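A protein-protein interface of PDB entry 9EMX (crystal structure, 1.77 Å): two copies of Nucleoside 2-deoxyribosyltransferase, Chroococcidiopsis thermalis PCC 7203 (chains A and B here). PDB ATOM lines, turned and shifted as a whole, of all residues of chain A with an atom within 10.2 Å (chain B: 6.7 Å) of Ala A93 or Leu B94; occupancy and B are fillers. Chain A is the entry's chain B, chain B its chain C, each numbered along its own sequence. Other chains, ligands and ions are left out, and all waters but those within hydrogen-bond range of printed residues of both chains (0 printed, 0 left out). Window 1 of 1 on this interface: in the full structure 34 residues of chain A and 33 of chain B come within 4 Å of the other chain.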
ATOM      1  N   LEU A  62      -8.854  -6.702   5.740  1.00  0.00           N
ATOM      2  CA  LEU A  62      -9.265  -6.859   4.350  1.00  0.00           C
ATOM      3  C   LEU A  62      -8.762  -5.700   3.490  1.00  0.00           C
ATOM      4  O   LEU A  62      -8.185  -5.914   2.417  1.00  0.00           O
ATOM      5  CB  LEU A  62     -10.794  -6.993   4.303  1.00  0.00           C
ATOM      6  CG  LEU A  62     -11.486  -7.359   2.988  1.00  0.00           C
ATOM      7  CD1 LEU A  62     -12.934  -7.758   3.263  1.00  0.00           C
ATOM      8  CD2 LEU A  62     -11.432  -6.217   2.006  1.00  0.00           C
ATOM      9  N   VAL A  65      -4.973  -5.762   2.850  1.00  0.00           N
ATOM     10  CA  VAL A  65      -4.562  -6.754   1.856  1.00  0.00           C
ATOM     11  C   VAL A  65      -4.884  -6.270   0.448  1.00  0.00           C
ATOM     12  O   VAL A  65      -4.100  -6.486  -0.489  1.00  0.00           O
ATOM     13  CB  VAL A  65      -5.205  -8.118   2.142  1.00  0.00           C
ATOM     14  CG1 VAL A  65      -4.843  -9.113   1.049  1.00  0.00           C
ATOM     15  CG2 VAL A  65      -4.698  -8.649   3.475  1.00  0.00           C
ATOM     16  N   LYS A  66      -6.028  -5.598   0.272  1.00  0.00           N
ATOM     17  CA  LYS A  66      -6.323  -4.987  -1.024  1.00  0.00           C
ATOM     18  C   LYS A  66      -5.284  -3.946  -1.406  1.00  0.00           C
ATOM     19  O   LYS A  66      -4.964  -3.802  -2.587  1.00  0.00           O
ATOM     20  CB  LYS A  66      -7.714  -4.348  -1.004  1.00  0.00           C
ATOM     21  CG  LYS A  66      -8.856  -5.358  -0.846  1.00  0.00           C
ATOM     22  CD  LYS A  66     -10.230  -4.694  -0.774  1.00  0.00           C
ATOM     23  CE  LYS A  66     -10.489  -3.825  -1.982  1.00  0.00           C
ATOM     24  NZ  LYS A  66     -10.435  -4.593  -3.254  1.00  0.00           N
ATOM     25  N   ILE A  71       2.079 -10.026   0.077  1.00  0.00           N
ATOM     26  CA  ILE A  71       1.834 -10.567   1.411  1.00  0.00           C
ATOM     27  C   ILE A  71       3.042 -11.402   1.818  1.00  0.00           C
ATOM     28  O   ILE A  71       3.607 -12.138   1.001  1.00  0.00           O
ATOM     29  CB  ILE A  71       0.530 -11.389   1.435  1.00  0.00           C
ATOM     30  CG1 ILE A  71       0.154 -11.796   2.855  1.00  0.00           C
ATOM     31  CG2 ILE A  71       0.652 -12.633   0.546  1.00  0.00           C
ATOM     32  CD1 ILE A  71      -1.207 -12.471   2.942  1.00  0.00           C
ATOM     33  N   MET A  85      -4.442 -17.915   6.352  1.00  0.00           N
ATOM     34  CA  MET A  85      -4.893 -18.585   5.132  1.00  0.00           C
ATOM     35  C   MET A  85      -5.964 -17.769   4.391  1.00  0.00           C
ATOM     36  O   MET A  85      -5.914 -17.667   3.162  1.00  0.00           O
ATOM     37  CB  MET A  85      -5.414 -19.983   5.475  1.00  0.00           C
ATOM     38  CG  MET A  85      -4.374 -20.951   6.104  1.00  0.00           C
ATOM     39  SD  MET A  85      -3.096 -21.279   4.814  1.00  0.00           S
ATOM     40  CE  MET A  85      -1.803 -20.136   5.349  1.00  0.00           C
ATOM     41  N   VAL A  86      -6.952 -17.199   5.103  1.00  0.00           N
ATOM     42  CA  VAL A  86      -7.928 -16.327   4.431  1.00  0.00           C
ATOM     43  C   VAL A  86      -7.199 -15.199   3.716  1.00  0.00           C
ATOM     44  O   VAL A  86      -7.449 -14.920   2.537  1.00  0.00           O
ATOM     45  CB  VAL A  86      -8.961 -15.751   5.420  1.00  0.00           C
ATOM     46  CG1 VAL A  86      -9.842 -14.666   4.709  1.00  0.00           C
ATOM     47  CG2 VAL A  86      -9.841 -16.844   6.040  1.00  0.00           C
ATOM     48  N   GLU A  87      -6.299 -14.517   4.432  1.00  0.00           N
ATOM     49  CA  GLU A  87      -5.627 -13.363   3.851  1.00  0.00           C
ATOM     50  C   GLU A  87      -4.750 -13.787   2.686  1.00  0.00           C
ATOM     51  O   GLU A  87      -4.680 -13.085   1.670  1.00  0.00           O
ATOM     52  CB  GLU A  87      -4.832 -12.630   4.930  1.00  0.00           C
ATOM     53  CG  GLU A  87      -5.739 -12.164   6.062  1.00  0.00           C
ATOM     54  CD  GLU A  87      -5.036 -11.540   7.257  1.00  0.00           C
ATOM     55  OE1 GLU A  87      -3.852 -11.851   7.532  1.00  0.00           O
ATOM     56  OE2 GLU A  87      -5.696 -10.739   7.953  1.00  0.00           O
ATOM     57  N   LEU A  88      -4.102 -14.952   2.801  1.00  0.00           N
ATOM     58  CA  LEU A  88      -3.339 -15.487   1.675  1.00  0.00           C
ATOM     59  C   LEU A  88      -4.240 -15.706   0.462  1.00  0.00           C
ATOM     60  O   LEU A  88      -3.862 -15.371  -0.673  1.00  0.00           O
ATOM     61  CB  LEU A  88      -2.639 -16.789   2.090  1.00  0.00           C
ATOM     62  CG  LEU A  88      -1.939 -17.621   1.006  1.00  0.00           C
ATOM     63  CD1 LEU A  88      -0.828 -16.826   0.326  1.00  0.00           C
ATOM     64  CD2 LEU A  88      -1.346 -18.909   1.592  1.00  0.00           C
ATOM     65  N   GLY A  89      -5.438 -16.257   0.685  1.00  0.00           N
ATOM     66  CA  GLY A  89      -6.373 -16.467  -0.409  1.00  0.00           C
ATOM     67  C   GLY A  89      -6.851 -15.160  -1.013  1.00  0.00           C
ATOM     68  O   GLY A  89      -6.942 -15.023  -2.240  1.00  0.00           O
ATOM     69  N   MET A  90      -7.173 -14.178  -0.168  1.00  0.00           N
ATOM     70  CA  MET A  90      -7.423 -12.840  -0.697  1.00  0.00           C
ATOM     71  C   MET A  90      -6.269 -12.375  -1.576  1.00  0.00           C
ATOM     72  O   MET A  90      -6.489 -11.903  -2.696  1.00  0.00           O
ATOM     73  CB  MET A  90      -7.648 -11.843   0.433  1.00  0.00           C
ATOM     74  CG  MET A  90      -8.869 -12.088   1.257  1.00  0.00           C
ATOM     75  SD  MET A  90      -8.820 -11.106   2.761  1.00  0.00           S
ATOM     76  CE  MET A  90     -10.509 -11.347   3.341  1.00  0.00           C
ATOM     77  N   ALA A  91      -5.028 -12.480  -1.079  1.00  0.00           N
ATOM     78  CA  ALA A  91      -3.888 -11.986  -1.848  1.00  0.00           C
ATOM     79  C   ALA A  91      -3.755 -12.715  -3.184  1.00  0.00           C
ATOM     80  O   ALA A  91      -3.457 -12.092  -4.211  1.00  0.00           O
ATOM     81  CB  ALA A  91      -2.592 -12.116  -1.047  1.00  0.00           C
ATOM     82  N   ILE A  92      -3.960 -14.034  -3.196  1.00  0.00           N
ATOM     83  CA  ILE A  92      -3.857 -14.777  -4.451  1.00  0.00           C
ATOM     84  C   ILE A  92      -4.889 -14.260  -5.452  1.00  0.00           C
ATOM     85  O   ILE A  92      -4.564 -13.969  -6.607  1.00  0.00           O
ATOM     86  CB  ILE A  92      -4.023 -16.287  -4.199  1.00  0.00           C
ATOM     87  CG1 ILE A  92      -2.898 -16.854  -3.323  1.00  0.00           C
ATOM     88  CG2 ILE A  92      -4.153 -17.087  -5.526  1.00  0.00           C
ATOM     89  CD1 ILE A  92      -3.252 -18.256  -2.791  1.00  0.00           C
ATOM     90  N   ALA A  93      -6.140 -14.102  -5.010  1.00  0.00           N
ATOM     91  CA  ALA A  93      -7.211 -13.687  -5.914  1.00  0.00           C
ATOM     92  C   ALA A  93      -7.004 -12.268  -6.432  1.00  0.00           C
ATOM     93  O   ALA A  93      -7.420 -11.947  -7.553  1.00  0.00           O
ATOM     94  CB  ALA A  93      -8.568 -13.796  -5.213  1.00  0.00           C
ATOM     95  N   LEU A  94      -6.383 -11.407  -5.632  1.00  0.00           N
ATOM     96  CA  LEU A  94      -6.083 -10.040  -6.020  1.00  0.00           C
ATOM     97  C   LEU A  94      -4.760  -9.906  -6.784  1.00  0.00           C
ATOM     98  O   LEU A  94      -4.280  -8.786  -6.965  1.00  0.00           O
ATOM     99  CB  LEU A  94      -6.077  -9.142  -4.778  1.00  0.00           C
ATOM    100  CG  LEU A  94      -7.412  -9.026  -4.043  1.00  0.00           C
ATOM    101  CD1 LEU A  94      -7.254  -8.303  -2.696  1.00  0.00           C
ATOM    102  CD2 LEU A  94      -8.447  -8.331  -4.932  1.00  0.00           C
ATOM    103  N   ASN A  95      -4.160 -11.008  -7.234  1.00  0.00           N
ATOM    104  CA  ASN A  95      -2.900 -10.972  -7.992  1.00  0.00           C
ATOM    105  C   ASN A  95      -1.781 -10.216  -7.272  1.00  0.00           C
ATOM    106  O   ASN A  95      -0.920  -9.603  -7.913  1.00  0.00           O
ATOM    107  CB  ASN A  95      -3.126 -10.382  -9.388  1.00  0.00           C
ATOM    108  CG  ASN A  95      -3.985 -11.280 -10.244  1.00  0.00           C
ATOM    109  OD1 ASN A  95      -3.741 -12.489 -10.325  1.00  0.00           O
ATOM    110  ND2 ASN A  95      -5.023 -10.717 -10.846  1.00  0.00           N
ATOM    111  N   LYS A  96      -1.748 -10.273  -5.943  1.00  0.00           N
ATOM    112  CA  LYS A  96      -0.620  -9.699  -5.224  1.00  0.00           C
ATOM    113  C   LYS A  96       0.588 -10.632  -5.294  1.00  0.00           C
ATOM    114  O   LYS A  96       0.472 -11.822  -5.599  1.00  0.00           O
ATOM    115  CB  LYS A  96      -0.980  -9.414  -3.767  1.00  0.00           C
ATOM    116  CG  LYS A  96      -2.240  -8.575  -3.571  1.00  0.00           C
ATOM    117  CD  LYS A  96      -2.091  -7.176  -4.143  1.00  0.00           C
ATOM    118  CE  LYS A  96      -3.257  -6.293  -3.713  1.00  0.00           C
ATOM    119  NZ  LYS A  96      -3.010  -4.891  -4.164  1.00  0.00           N
ATOM    120  N   ALA A  97       1.766 -10.067  -5.021  1.00  0.00           N
ATOM    121  CA  ALA A  97       2.966 -10.881  -4.873  1.00  0.00           C
ATOM    122  C   ALA A  97       2.858 -11.694  -3.586  1.00  0.00           C
ATOM    123  O   ALA A  97       2.408 -11.177  -2.561  1.00  0.00           O
ATOM    124  CB  ALA A  97       4.217  -9.997  -4.836  1.00  0.00           C
ATOM    125  N   ILE A  98       3.240 -12.969  -3.649  1.00  0.00           N
ATOM    126  CA  ILE A  98       3.065 -13.914  -2.530  1.00  0.00           C
ATOM    127  C   ILE A  98       4.423 -14.409  -2.068  1.00  0.00           C
ATOM    128  O   ILE A  98       5.185 -14.965  -2.867  1.00  0.00           O
ATOM    129  CB  ILE A  98       2.201 -15.138  -2.909  1.00  0.00           C
ATOM    130  CG1 ILE A  98       0.872 -14.736  -3.573  1.00  0.00           C
ATOM    131  CG2 ILE A  98       1.933 -16.053  -1.672  1.00  0.00           C
ATOM    132  CD1 ILE A  98      -0.105 -14.008  -2.672  1.00  0.00           C
ATOM    133  N   MET A 119      -3.093 -25.891  -1.872  1.00  0.00           N
ATOM    134  CA  MET A 119      -3.789 -24.647  -2.229  1.00  0.00           C
ATOM    135  C   MET A 119      -3.005 -23.411  -1.795  1.00  0.00           C
ATOM    136  O   MET A 119      -3.214 -22.322  -2.354  1.00  0.00           O
ATOM    137  CB  MET A 119      -5.206 -24.619  -1.637  1.00  0.00           C
ATOM    138  CG  MET A 119      -6.189 -25.568  -2.340  1.00  0.00           C
ATOM    139  SD  MET A 119      -6.389 -25.158  -4.077  1.00  0.00           S
ATOM    140  CE  MET A 119      -6.943 -23.509  -3.885  1.00  0.00           C
ATOM    141  N   LEU A 120      -2.096 -23.554  -0.826  1.00  0.00           N
ATOM    142  CA  LEU A 120      -1.271 -22.419  -0.417  1.00  0.00           C
ATOM    143  C   LEU A 120      -0.352 -21.946  -1.534  1.00  0.00           C
ATOM    144  O   LEU A 120       0.107 -20.800  -1.500  1.00  0.00           O
ATOM    145  CB  LEU A 120      -0.424 -22.786   0.812  1.00  0.00           C
ATOM    146  CG  LEU A 120      -1.097 -22.740   2.179  1.00  0.00           C
ATOM    147  CD1 LEU A 120      -2.121 -23.849   2.315  1.00  0.00           C
ATOM    148  CD2 LEU A 120      -0.061 -22.821   3.317  1.00  0.00           C
ATOM    149  N   ALA A 122      -1.147 -22.076  -4.863  1.00  0.00           N
ATOM    150  CA  ALA A 122      -1.919 -21.810  -6.072  1.00  0.00           C
ATOM    151  C   ALA A 122      -1.598 -20.454  -6.697  1.00  0.00           C
ATOM    152  O   ALA A 122      -1.815 -20.267  -7.901  1.00  0.00           O
ATOM    153  CB  ALA A 122      -3.412 -21.879  -5.753  1.00  0.00           C
ATOM    154  N   GLY A 123      -1.128 -19.490  -5.906  1.00  0.00           N
ATOM    155  CA  GLY A 123      -0.751 -18.191  -6.420  1.00  0.00           C
ATOM    156  C   GLY A 123       0.680 -18.078  -6.898  1.00  0.00           C
ATOM    157  O   GLY A 123       1.054 -17.032  -7.426  1.00  0.00           O
ATOM    158  N   LEU A 124       1.496 -19.121  -6.717  1.00  0.00           N
ATOM    159  CA  LEU A 124       2.894 -19.140  -7.132  1.00  0.00           C
ATOM    160  C   LEU A 124       3.056 -19.855  -8.460  1.00  0.00           C
ATOM    161  O   LEU A 124       2.226 -20.687  -8.837  1.00  0.00           O
ATOM    162  CB  LEU A 124       3.753 -19.843  -6.063  1.00  0.00           C
ATOM    163  CG  LEU A 124       3.735 -19.180  -4.686  1.00  0.00           C
ATOM    164  CD1 LEU A 124       4.610 -19.962  -3.700  1.00  0.00           C
ATOM    165  CD2 LEU A 124       4.217 -17.741  -4.804  1.00  0.00           C
ATOM    166  N   LEU B  62      -8.542 -23.157  -8.020  1.00  0.00           N
ATOM    167  CA  LEU B  62      -8.549 -21.708  -8.139  1.00  0.00           C
ATOM    168  C   LEU B  62      -9.534 -21.251  -9.212  1.00  0.00           C
ATOM    169  O   LEU B  62     -10.282 -20.289  -9.006  1.00  0.00           O
ATOM    170  CB  LEU B  62      -7.129 -21.220  -8.422  1.00  0.00           C
ATOM    171  CG  LEU B  62      -6.887 -19.738  -8.722  1.00  0.00           C
ATOM    172  CD1 LEU B  62      -5.426 -19.387  -8.473  1.00  0.00           C
ATOM    173  CD2 LEU B  62      -7.248 -19.419 -10.149  1.00  0.00           C
ATOM    174  N   VAL B  65     -13.260 -21.576  -8.178  1.00  0.00           N
ATOM    175  CA  VAL B  65     -13.692 -20.499  -7.295  1.00  0.00           C
ATOM    176  C   VAL B  65     -13.897 -19.209  -8.086  1.00  0.00           C
ATOM    177  O   VAL B  65     -14.838 -18.449  -7.820  1.00  0.00           O
ATOM    178  CB  VAL B  65     -12.694 -20.318  -6.139  1.00  0.00           C
ATOM    179  CG1 VAL B  65     -13.103 -19.145  -5.239  1.00  0.00           C
ATOM    180  CG2 VAL B  65     -12.583 -21.609  -5.319  1.00  0.00           C
ATOM    181  N   LYS B  66     -13.036 -18.940  -9.075  1.00  0.00           N
ATOM    182  CA  LYS B  66     -13.249 -17.777  -9.930  1.00  0.00           C
ATOM    183  C   LYS B  66     -14.569 -17.876 -10.684  1.00  0.00           C
ATOM    184  O   LYS B  66     -15.197 -16.854 -10.965  1.00  0.00           O
ATOM    185  CB  LYS B  66     -12.104 -17.619 -10.934  1.00  0.00           C
ATOM    186  CG  LYS B  66     -10.741 -17.319 -10.317  1.00  0.00           C
ATOM    187  CD  LYS B  66      -9.731 -17.011 -11.409  1.00  0.00           C
ATOM    188  CE  LYS B  66     -10.346 -16.086 -12.448  1.00  0.00           C
ATOM    189  NZ  LYS B  66      -9.322 -15.435 -13.332  1.00  0.00           N
ATOM    190  N   ASN B  67     -15.011 -19.095 -11.006  1.00  0.00           N
ATOM    191  CA  ASN B  67     -16.153 -19.313 -11.891  1.00  0.00           C
ATOM    192  C   ASN B  67     -17.440 -19.676 -11.172  1.00  0.00           C
ATOM    193  O   ASN B  67     -18.489 -19.754 -11.817  1.00  0.00           O
ATOM    194  CB  ASN B  67     -15.820 -20.407 -12.897  1.00  0.00           C
ATOM    195  CG  ASN B  67     -14.833 -19.940 -13.907  1.00  0.00           C
ATOM    196  OD1 ASN B  67     -14.815 -18.759 -14.242  1.00  0.00           O
ATOM    197  ND2 ASN B  67     -13.975 -20.843 -14.387  1.00  0.00           N
ATOM    198  N   GLY B  89     -10.893 -17.280   1.372  1.00  0.00           N
ATOM    199  CA  GLY B  89     -10.228 -16.007   1.132  1.00  0.00           C
ATOM    200  C   GLY B  89     -10.322 -15.560  -0.315  1.00  0.00           C
ATOM    201  O   GLY B  89     -10.632 -14.401  -0.598  1.00  0.00           O
ATOM    202  N   MET B  90     -10.055 -16.474  -1.254  1.00  0.00           N
ATOM    203  CA  MET B  90     -10.277 -16.148  -2.660  1.00  0.00           C
ATOM    204  C   MET B  90     -11.713 -15.701  -2.906  1.00  0.00           C
ATOM    205  O   MET B  90     -11.942 -14.710  -3.604  1.00  0.00           O
ATOM    206  CB  MET B  90      -9.949 -17.344  -3.554  1.00  0.00           C
ATOM    207  CG  MET B  90      -8.497 -17.787  -3.536  1.00  0.00           C
ATOM    208  SD  MET B  90      -8.412 -19.476  -4.158  1.00  0.00           S
ATOM    209  CE  MET B  90      -6.628 -19.596  -4.411  1.00  0.00           C
ATOM    210  N   ALA B  91     -12.698 -16.430  -2.363  1.00  0.00           N
ATOM    211  CA  ALA B  91     -14.098 -16.090  -2.630  1.00  0.00           C
ATOM    212  C   ALA B  91     -14.428 -14.689  -2.120  1.00  0.00           C
ATOM    213  O   ALA B  91     -15.099 -13.905  -2.807  1.00  0.00           O
ATOM    214  CB  ALA B  91     -15.031 -17.129  -1.988  1.00  0.00           C
ATOM    215  N   ILE B  92     -13.953 -14.355  -0.920  1.00  0.00           N
ATOM    216  CA  ILE B  92     -14.194 -13.032  -0.356  1.00  0.00           C
ATOM    217  C   ILE B  92     -13.661 -11.942  -1.283  1.00  0.00           C
ATOM    218  O   ILE B  92     -14.356 -10.963  -1.587  1.00  0.00           O
ATOM    219  CB  ILE B  92     -13.558 -12.932   1.038  1.00  0.00           C
ATOM    220  CG1 ILE B  92     -14.241 -13.916   2.002  1.00  0.00           C
ATOM    221  CG2 ILE B  92     -13.610 -11.492   1.540  1.00  0.00           C
ATOM    222  CD1 ILE B  92     -13.650 -13.897   3.389  1.00  0.00           C
ATOM    223  N   ALA B  93     -12.411 -12.088  -1.732  1.00  0.00           N
ATOM    224  CA  ALA B  93     -11.798 -11.061  -2.571  1.00  0.00           C
ATOM    225  C   ALA B  93     -12.506 -10.947  -3.910  1.00  0.00           C
ATOM    226  O   ALA B  93     -12.518  -9.871  -4.523  1.00  0.00           O
ATOM    227  CB  ALA B  93     -10.314 -11.372  -2.792  1.00  0.00           C
ATOM    228  N   LEU B  94     -13.086 -12.038  -4.389  1.00  0.00           N
ATOM    229  CA  LEU B  94     -13.747 -12.022  -5.681  1.00  0.00           C
ATOM    230  C   LEU B  94     -15.236 -11.692  -5.570  1.00  0.00           C
ATOM    231  O   LEU B  94     -15.969 -11.875  -6.542  1.00  0.00           O
ATOM    232  CB  LEU B  94     -13.538 -13.368  -6.387  1.00  0.00           C
ATOM    233  CG  LEU B  94     -12.099 -13.732  -6.788  1.00  0.00           C
ATOM    234  CD1 LEU B  94     -11.973 -15.209  -7.153  1.00  0.00           C
ATOM    235  CD2 LEU B  94     -11.606 -12.866  -7.949  1.00  0.00           C
ATOM    236  N   ASN B  95     -15.695 -11.225  -4.405  1.00  0.00           N
ATOM    237  CA  ASN B  95     -17.097 -10.858  -4.184  1.00  0.00           C
ATOM    238  C   ASN B  95     -18.071 -11.975  -4.564  1.00  0.00           C
ATOM    239  O   ASN B  95     -19.168 -11.719  -5.061  1.00  0.00           O
ATOM    240  CB  ASN B  95     -17.449  -9.566  -4.935  1.00  0.00           C
ATOM    241  CG  ASN B  95     -16.564  -8.403  -4.534  1.00  0.00           C
ATOM    242  OD1 ASN B  95     -16.576  -7.969  -3.374  1.00  0.00           O
ATOM    243  ND2 ASN B  95     -15.778  -7.897  -5.489  1.00  0.00           N
ATOM    244  N   LYS B  96     -17.680 -13.221  -4.335  1.00  0.00           N
ATOM    245  CA  LYS B  96     -18.641 -14.305  -4.410  1.00  0.00           C
ATOM    246  C   LYS B  96     -19.543 -14.274  -3.180  1.00  0.00           C
ATOM    247  O   LYS B  96     -19.217 -13.663  -2.158  1.00  0.00           O
ATOM    248  CB  LYS B  96     -17.923 -15.651  -4.522  1.00  0.00           C
ATOM    249  CG  LYS B  96     -16.902 -15.729  -5.667  1.00  0.00           C
ATOM    250  CD  LYS B  96     -17.523 -15.376  -7.025  1.00  0.00           C
ATOM    251  CE  LYS B  96     -16.602 -15.766  -8.162  1.00  0.00           C
ATOM    252  NZ  LYS B  96     -17.261 -15.601  -9.494  1.00  0.00           N
ATOM    253  N   ALA B  97     -20.701 -14.930  -3.287  1.00  0.00           N
ATOM    254  CA  ALA B  97     -21.540 -15.120  -2.114  1.00  0.00           C
ATOM    255  C   ALA B  97     -20.882 -16.134  -1.182  1.00  0.00           C
ATOM    256  O   ALA B  97     -20.312 -17.133  -1.637  1.00  0.00           O
ATOM    257  CB  ALA B  97     -22.933 -15.609  -2.511  1.00  0.00           C
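Of the 13 printed residues of chain B, 6 touch a printed residue of chain A.
Printed residues of chain B that touch a printed residue of chain A: Leu B62, Gly B89, Met B90, Ile B92, Ala B93 and Leu B94.
Hydrophobic or aromatic side chains of chain B that line the printed part of chain A: Leu B62, Met B90, Ile B92, Ala B93 and Leu B94.
Among the printed residues, no Asp or Glu carboxylate lies within 4 Å of a Lys or Arg side-chain nitrogen of the other chain.
Gly B89 touches Val A86.
C of Gly B89 touches C of Gly A89, 3.6 Å away.
Gly A89 touches Met B90.
N of Met A90 touches N of Met B90, 3.8 Å away.
CA of Met A90 touches CB of Ala B93 (3.9 Å).
CG2 of Ile A92 touches CE of Met B90, at 3.7 Å.
Met B90 touches Ala A93.
Ala B93 touches Ala A93.
Ala B93 touches Leu A94.
Leu B62 touches Ala A122.
Gly A89 touches Met B90, and with the chains exchanged Met A90 touches Gly B89.
Met A90 touches Ile B92, and with the chains exchanged Ile A92 touches Met B90.
Met A90 touches Ala B93, and with the chains exchanged Ala A93 touches Met B90.
Ile A92 touches Leu B62, but with the chains exchanged Leu A62 does not touch Ile B92 (4.2 Å).
Positions printed for both chains: 62, 65, 66, 89, 90, 91, 92, 93, 94, 95, 96 and 97.
Of the 15 pairs that touch across the chains among the printed residues, 11 have their exchanged pair printed and touching as well.
N of Met A90 sits close to O of Gly B89, 3.5 Å away.
Ala A93 touches just these residues of chain B: Met B90 (3.8 Å), Ala B93 (3.8 Å) and Leu B94 (3.9 Å).
Of chain A, only Ala A93 (3.9 Å) comes within 4 Å of Leu B94.
Of chain A, only Gly A89, Met A90, Ile A92, Ala A93 and Met A119 come within 4 Å of Met B90.
Ala B93 touches just these residues of chain A: Met A90 (3.9 Å), Ala A93 (3.8 Å) and Leu A94 (3.9 Å).
No residue of chain A comes within 4 Å of Asn B95.
No residue of chain A comes within 4 Å of Lys B96.
Of the printed residues of chain B, Met A90 touches Gly B89, Met B90, Ile B92 and Ala B93.
Printed residues of chain B within 4 Å of Ala A122: Leu B62.
Of the printed residues of chain B, Gly A89 touches Gly B89 (3.6 Å) and Met B90 (3.4 Å).
Printed residues of chain A within 4 Å of Leu B62: Ile A92 and Ala A122.
The nearest residue of chain A that does not touch Leu B94 is Leu A94 (5.9 Å).
The nearest printed residue of chain B that does not touch Leu A94 is Leu B94 (5.9 Å).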
